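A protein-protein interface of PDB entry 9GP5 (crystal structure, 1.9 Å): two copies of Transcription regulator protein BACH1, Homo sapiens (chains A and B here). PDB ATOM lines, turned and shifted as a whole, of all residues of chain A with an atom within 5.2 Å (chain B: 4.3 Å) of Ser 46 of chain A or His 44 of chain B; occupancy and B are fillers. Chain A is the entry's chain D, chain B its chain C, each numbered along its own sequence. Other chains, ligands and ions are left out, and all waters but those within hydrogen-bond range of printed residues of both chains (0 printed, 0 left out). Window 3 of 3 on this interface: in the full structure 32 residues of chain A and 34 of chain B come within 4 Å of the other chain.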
ATOM      1  N   ASP A  31      -3.918  16.901 -10.971  1.00  0.00           N
ATOM      2  CA  ASP A  31      -4.786  15.874 -11.521  1.00  0.00           C
ATOM      3  C   ASP A  31      -4.647  14.531 -10.789  1.00  0.00           C
ATOM      4  O   ASP A  31      -5.300  13.584 -11.173  1.00  0.00           O
ATOM      5  CB  ASP A  31      -4.486  15.754 -13.022  1.00  0.00           C
ATOM      6  CG  ASP A  31      -3.010  15.430 -13.263  1.00  0.00           C
ATOM      7  OD1 ASP A  31      -2.608  14.349 -12.808  1.00  0.00           O
ATOM      8  OD2 ASP A  31      -2.245  16.302 -13.751  1.00  0.00           O
ATOM      9  N   HIS A  44       0.818  16.357 -10.377  1.00  0.00           N
ATOM     10  CA  HIS A  44       0.494  16.120 -11.770  1.00  0.00           C
ATOM     11  C   HIS A  44       0.984  14.723 -12.158  1.00  0.00           C
ATOM     12  O   HIS A  44       2.142  14.384 -11.874  1.00  0.00           O
ATOM     13  CB  HIS A  44       1.200  17.120 -12.694  1.00  0.00           C
ATOM     14  CG  HIS A  44       1.115  18.575 -12.337  1.00  0.00           C
ATOM     15  ND1 HIS A  44       1.969  19.181 -11.435  1.00  0.00           N
ATOM     16  CD2 HIS A  44       0.271  19.521 -12.782  1.00  0.00           C
ATOM     17  CE1 HIS A  44       1.626  20.468 -11.328  1.00  0.00           C
ATOM     18  NE2 HIS A  44       0.616  20.718 -12.167  1.00  0.00           N
ATOM     19  N   ARG A  45       0.080  13.901 -12.712  1.00  0.00           N
ATOM     20  CA  ARG A  45       0.412  12.519 -13.004  1.00  0.00           C
ATOM     21  C   ARG A  45       1.570  12.494 -14.003  1.00  0.00           C
ATOM     22  O   ARG A  45       2.397  11.609 -13.935  1.00  0.00           O
ATOM     23  CB  ARG A  45      -0.830  11.767 -13.449  1.00  0.00           C
ATOM     24  CG  ARG A  45      -1.339  12.103 -14.844  1.00  0.00           C
ATOM     25  CD  ARG A  45      -2.648  11.374 -15.007  1.00  0.00           C
ATOM     26  NE  ARG A  45      -3.708  11.843 -14.109  1.00  0.00           N
ATOM     27  CZ  ARG A  45      -4.965  11.421 -14.170  1.00  0.00           C
ATOM     28  NH1 ARG A  45      -5.917  12.050 -13.519  1.00  0.00           N
ATOM     29  NH2 ARG A  45      -5.291  10.383 -14.929  1.00  0.00           N
ATOM     30  N   SER A  46       1.620  13.471 -14.927  1.00  0.00           N
ATOM     31  CA  SER A  46       2.679  13.528 -15.932  1.00  0.00           C
ATOM     32  C   SER A  46       4.050  13.680 -15.291  1.00  0.00           C
ATOM     33  O   SER A  46       5.010  13.032 -15.687  1.00  0.00           O
ATOM     34  CB  SER A  46       2.396  14.623 -16.914  1.00  0.00           C
ATOM     35  OG  SER A  46       2.207  15.852 -16.249  1.00  0.00           O
ATOM     36  N   VAL A  47       4.166  14.522 -14.269  1.00  0.00           N
ATOM     37  CA  VAL A  47       5.441  14.775 -13.625  1.00  0.00           C
ATOM     38  C   VAL A  47       5.824  13.549 -12.778  1.00  0.00           C
ATOM     39  O   VAL A  47       6.997  13.133 -12.798  1.00  0.00           O
ATOM     40  CB  VAL A  47       5.401  16.052 -12.764  1.00  0.00           C
ATOM     41  CG1 VAL A  47       6.659  16.145 -11.893  1.00  0.00           C
ATOM     42  CG2 VAL A  47       5.139  17.307 -13.579  1.00  0.00           C
ATOM     43  N   LEU A  48       4.862  12.981 -12.032  1.00  0.00           N
ATOM     44  CA  LEU A  48       5.144  11.809 -11.209  1.00  0.00           C
ATOM     45  C   LEU A  48       5.615  10.649 -12.071  1.00  0.00           C
ATOM     46  O   LEU A  48       6.610   9.998 -11.750  1.00  0.00           O
ATOM     47  CB  LEU A  48       3.906  11.396 -10.437  1.00  0.00           C
ATOM     48  CG  LEU A  48       3.474  12.400  -9.368  1.00  0.00           C
ATOM     49  CD1 LEU A  48       2.384  11.760  -8.518  1.00  0.00           C
ATOM     50  CD2 LEU A  48       4.644  12.851  -8.507  1.00  0.00           C
ATOM     51  N   ALA A  49       4.951  10.450 -13.203  1.00  0.00           N
ATOM     52  CA  ALA A  49       5.351   9.378 -14.108  1.00  0.00           C
ATOM     53  C   ALA A  49       6.727   9.650 -14.694  1.00  0.00           C
ATOM     54  O   ALA A  49       7.462   8.697 -14.988  1.00  0.00           O
ATOM     55  CB  ALA A  49       4.333   9.235 -15.209  1.00  0.00           C
ATOM     56  N   ALA A  50       7.053  10.927 -14.909  1.00  0.00           N
ATOM     57  CA  ALA A  50       8.352  11.319 -15.440  1.00  0.00           C
ATOM     58  C   ALA A  50       9.489  11.064 -14.447  1.00  0.00           C
ATOM     59  O   ALA A  50      10.626  10.786 -14.858  1.00  0.00           O
ATOM     60  CB  ALA A  50       8.361  12.751 -15.853  1.00  0.00           C
ATOM     61  N   LEU B  20       8.205  15.059 -20.492  1.00  0.00           N
ATOM     62  CA  LEU B  20       6.922  15.631 -20.850  1.00  0.00           C
ATOM     63  C   LEU B  20       6.813  15.788 -22.360  1.00  0.00           C
ATOM     64  O   LEU B  20       5.737  15.587 -22.907  1.00  0.00           O
ATOM     65  CB  LEU B  20       6.721  16.985 -20.170  1.00  0.00           C
ATOM     66  CG  LEU B  20       6.664  16.994 -18.640  1.00  0.00           C
ATOM     67  CD1 LEU B  20       6.654  18.412 -18.126  1.00  0.00           C
ATOM     68  CD2 LEU B  20       5.488  16.230 -18.146  1.00  0.00           C
ATOM     69  N   GLN B  23       5.910  12.367 -23.685  1.00  0.00           N
ATOM     70  CA  GLN B  23       4.479  12.123 -23.452  1.00  0.00           C
ATOM     71  C   GLN B  23       3.620  12.851 -24.476  1.00  0.00           C
ATOM     72  O   GLN B  23       2.687  12.278 -25.061  1.00  0.00           O
ATOM     73  CB  GLN B  23       4.115  12.637 -22.062  1.00  0.00           C
ATOM     74  CG  GLN B  23       4.686  11.737 -20.969  1.00  0.00           C
ATOM     75  CD  GLN B  23       4.425  12.322 -19.605  1.00  0.00           C
ATOM     76  OE1 GLN B  23       3.556  13.188 -19.442  1.00  0.00           O
ATOM     77  NE2 GLN B  23       5.206  11.881 -18.625  1.00  0.00           N
ATOM     78  N   ARG B  24       3.939  14.132 -24.722  1.00  0.00           N
ATOM     79  CA  ARG B  24       3.213  14.911 -25.723  1.00  0.00           C
ATOM     80  C   ARG B  24       3.256  14.208 -27.085  1.00  0.00           C
ATOM     81  O   ARG B  24       2.221  13.994 -27.762  1.00  0.00           O
ATOM     82  CB  ARG B  24       3.790  16.327 -25.840  1.00  0.00           C
ATOM     83  CG  ARG B  24       3.160  17.173 -26.943  1.00  0.00           C
ATOM     84  CD  ARG B  24       3.819  18.508 -27.030  1.00  0.00           C
ATOM     85  NE  ARG B  24       5.162  18.462 -27.612  1.00  0.00           N
ATOM     86  CZ  ARG B  24       5.395  18.566 -28.907  1.00  0.00           C
ATOM     87  NH1 ARG B  24       6.625  18.571 -29.360  1.00  0.00           N
ATOM     88  NH2 ARG B  24       4.387  18.743 -29.732  1.00  0.00           N
ATOM     89  N   LEU B  29      -0.654  10.448 -21.268  1.00  0.00           N
ATOM     90  CA  LEU B  29      -0.754  11.305 -20.082  1.00  0.00           C
ATOM     91  C   LEU B  29      -0.955  12.793 -20.431  1.00  0.00           C
ATOM     92  O   LEU B  29      -0.726  13.671 -19.605  1.00  0.00           O
ATOM     93  CB  LEU B  29       0.481  11.144 -19.204  1.00  0.00           C
ATOM     94  CG  LEU B  29       0.748   9.732 -18.696  1.00  0.00           C
ATOM     95  CD1 LEU B  29       1.834   9.749 -17.628  1.00  0.00           C
ATOM     96  CD2 LEU B  29      -0.516   9.104 -18.133  1.00  0.00           C
ATOM     97  N   CYS B  30      -1.532  13.062 -21.588  1.00  0.00           N
ATOM     98  CA  CYS B  30      -1.907  14.403 -21.981  1.00  0.00           C
ATOM     99  C   CYS B  30      -3.344  14.656 -21.520  1.00  0.00           C
ATOM    100  O   CYS B  30      -4.062  13.734 -21.148  1.00  0.00           O
ATOM    101  CB  CYS B  30      -1.768  14.551 -23.490  1.00  0.00           C
ATOM    102  SG  CYS B  30      -0.034  14.729 -23.983  1.00  0.00           S
ATOM    103  N   ASP B  31      -3.779  15.926 -21.507  1.00  0.00           N
ATOM    104  CA  ASP B  31      -5.070  16.248 -20.891  1.00  0.00           C
ATOM    105  C   ASP B  31      -5.771  17.422 -21.587  1.00  0.00           C
ATOM    106  O   ASP B  31      -6.883  17.786 -21.201  1.00  0.00           O
ATOM    107  CB  ASP B  31      -4.852  16.530 -19.391  1.00  0.00           C
ATOM    108  CG  ASP B  31      -3.826  17.661 -19.200  1.00  0.00           C
ATOM    109  OD1 ASP B  31      -4.131  18.766 -19.682  1.00  0.00           O
ATOM    110  OD2 ASP B  31      -2.688  17.404 -18.745  1.00  0.00           O
ATOM    111  N   VAL B  32      -5.212  17.954 -22.675  1.00  0.00           N
ATOM    112  CA  VAL B  32      -5.874  18.999 -23.430  1.00  0.00           C
ATOM    113  C   VAL B  32      -5.546  18.790 -24.904  1.00  0.00           C
ATOM    114  O   VAL B  32      -4.429  18.402 -25.266  1.00  0.00           O
ATOM    115  CB  VAL B  32      -5.450  20.395 -22.906  1.00  0.00           C
ATOM    116  CG1 VAL B  32      -3.977  20.634 -23.031  1.00  0.00           C
ATOM    117  CG2 VAL B  32      -6.230  21.560 -23.531  1.00  0.00           C
ATOM    118  N   ALA B  43      -1.451  18.143 -25.504  1.00  0.00           N
ATOM    119  CA  ALA B  43      -0.531  18.750 -24.583  1.00  0.00           C
ATOM    120  C   ALA B  43      -1.078  18.560 -23.181  1.00  0.00           C
ATOM    121  O   ALA B  43      -2.060  17.839 -22.982  1.00  0.00           O
ATOM    122  CB  ALA B  43      -0.325  20.191 -24.897  1.00  0.00           C
ATOM    123  N   HIS B  44      -0.315  19.137 -22.241  1.00  0.00           N
ATOM    124  CA  HIS B  44      -0.649  19.137 -20.839  1.00  0.00           C
ATOM    125  C   HIS B  44      -1.062  20.563 -20.443  1.00  0.00           C
ATOM    126  O   HIS B  44      -0.331  21.510 -20.740  1.00  0.00           O
ATOM    127  CB  HIS B  44       0.564  18.748 -19.987  1.00  0.00           C
ATOM    128  CG  HIS B  44       1.282  17.492 -20.368  1.00  0.00           C
ATOM    129  ND1 HIS B  44       2.307  17.487 -21.315  1.00  0.00           N
ATOM    130  CD2 HIS B  44       1.187  16.261 -19.852  1.00  0.00           C
ATOM    131  CE1 HIS B  44       2.794  16.226 -21.392  1.00  0.00           C
ATOM    132  NE2 HIS B  44       2.155  15.469 -20.497  1.00  0.00           N
ATOM    133  N   ARG B  45      -2.246  20.707 -19.834  1.00  0.00           N
ATOM    134  CA  ARG B  45      -2.764  22.037 -19.540  1.00  0.00           C
ATOM    135  C   ARG B  45      -1.802  22.732 -18.569  1.00  0.00           C
ATOM    136  O   ARG B  45      -1.606  23.927 -18.683  1.00  0.00           O
ATOM    137  CB  ARG B  45      -4.196  21.929 -19.056  1.00  0.00           C
ATOM    138  CG  ARG B  45      -4.353  21.390 -17.640  1.00  0.00           C
ATOM    139  CD  ARG B  45      -5.832  21.161 -17.370  1.00  0.00           C
ATOM    140  NE  ARG B  45      -6.430  20.179 -18.276  1.00  0.00           N
ATOM    141  CZ  ARG B  45      -7.664  19.703 -18.140  1.00  0.00           C
ATOM    142  NH1 ARG B  45      -8.476  20.238 -17.242  1.00  0.00           N
ATOM    143  NH2 ARG B  45      -8.109  18.714 -18.896  1.00  0.00           N
ATOM    144  N   SER B  46      -1.171  21.960 -17.660  1.00  0.00           N
ATOM    145  CA  SER B  46      -0.211  22.524 -16.709  1.00  0.00           C
ATOM    146  C   SER B  46       0.946  23.213 -17.415  1.00  0.00           C
ATOM    147  O   SER B  46       1.382  24.292 -17.027  1.00  0.00           O
ATOM    148  CB  SER B  46       0.283  21.460 -15.776  1.00  0.00           C
ATOM    149  OG  SER B  46       0.789  20.364 -16.522  1.00  0.00           O
ATOM    150  N   VAL B  47       1.486  22.569 -18.448  1.00  0.00           N
ATOM    151  CA  VAL B  47       2.628  23.098 -19.157  1.00  0.00           C
ATOM    152  C   VAL B  47       2.221  24.324 -19.993  1.00  0.00           C
ATOM    153  O   VAL B  47       2.953  25.337 -20.008  1.00  0.00           O
ATOM    154  CB  VAL B  47       3.344  22.039 -20.005  1.00  0.00           C
ATOM    155  CG1 VAL B  47       4.374  22.699 -20.945  1.00  0.00           C
ATOM    156  CG2 VAL B  47       3.911  20.903 -19.151  1.00  0.00           C
ATOM    157  N   LEU B  48       1.080  24.235 -20.688  1.00  0.00           N
ATOM    158  CA  LEU B  48       0.584  25.354 -21.496  1.00  0.00           C
ATOM    159  C   LEU B  48       0.383  26.583 -20.628  1.00  0.00           C
ATOM    160  O   LEU B  48       0.799  27.665 -21.009  1.00  0.00           O
ATOM    161  CB  LEU B  48      -0.726  24.963 -22.167  1.00  0.00           C
ATOM    162  CG  LEU B  48      -0.576  23.878 -23.241  1.00  0.00           C
ATOM    163  CD1 LEU B  48      -1.879  23.786 -24.030  1.00  0.00           C
ATOM    164  CD2 LEU B  48       0.595  24.126 -24.174  1.00  0.00           C
ATOM    165  N   TYR B  88       8.059  22.789 -24.946  1.00  0.00           N
ATOM    166  CA  TYR B  88       8.404  21.443 -24.498  1.00  0.00           C
ATOM    167  C   TYR B  88       9.866  21.061 -24.643  1.00  0.00           C
ATOM    168  O   TYR B  88      10.235  19.956 -24.196  1.00  0.00           O
ATOM    169  CB  TYR B  88       7.516  20.425 -25.212  1.00  0.00           C
ATOM    170  CG  TYR B  88       6.147  20.263 -24.593  1.00  0.00           C
ATOM    171  CD1 TYR B  88       5.104  21.128 -24.880  1.00  0.00           C
ATOM    172  CD2 TYR B  88       5.962  19.312 -23.620  1.00  0.00           C
ATOM    173  CE1 TYR B  88       3.853  20.940 -24.338  1.00  0.00           C
ATOM    174  CE2 TYR B  88       4.735  19.160 -23.003  1.00  0.00           C
ATOM    175  CZ  TYR B  88       3.681  19.968 -23.355  1.00  0.00           C
ATOM    176  OH  TYR B  88       2.498  19.683 -22.750  1.00  0.00           O
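NE2 of Gln 23 of chain B sits at hydrogen-bond distance from O of Ser 46 of chain A (3.2 Å).
Of the printed residues of chain B, Ala 49 of chain A touches Leu 29. Of the printed residues of chain A, Leu 20 of chain B touches Ser 46. Of the printed residues of chain A, Ser 46 of chain B touches His 44 (3.6 Å). Of the printed residues of chain B, His 44 of chain A touches Ser 46 (3.6 Å). Printed residues of chain A within 4 Å of Gln 23 of chain B: Ser 46. The nearest residue of chain B that does not touch Ser 46 of chain A is Leu 29 of chain B (4.2 Å).
Among the printed residues, merely in contact across the chains: His 44 of chain A with Ser 46 of chain B, Ser 46 of chain A with Leu 20 of chain B, Ser 46 of chain A with His 44 of chain B and Ala 49 of chain A with Leu 29 of chain B.
His 44 of chain A touches Ser 46 of chain B, and with the chains exchanged Ser 46 of chain A touches His 44 of chain B. Of the 5 pairs that touch across the chains among the printed residues, 2 have their exchanged pair printed and touching as well.
A ring nitrogen (ND1) of His 44 of chain B sits at hydrogen-bond distance from the side-chain hydroxyl (OH) of Tyr 88 of chain B (2.6 Å). The side-chain amide oxygen of Gln 23 of chain B sits at hydrogen-bond distance from a ring nitrogen (NE2) of His 44 of chain B, 2.9 Å away.
Along chain A the printed residues that touch a printed residue of chain B span positions 44 to 49. Of the 14 printed residues of chain B, 5 touch a printed residue of chain A. Printed residues of chain B that touch a printed residue of chain A: Leu 20, Gln 23, Leu 29, His 44 and Ser 46. Among the printed residues, 5 pairs touch across the chains. Among the printed residues, no Asp or Glu carboxylate lies within 4 Å of a Lys or Arg side-chain nitrogen of the other chain.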
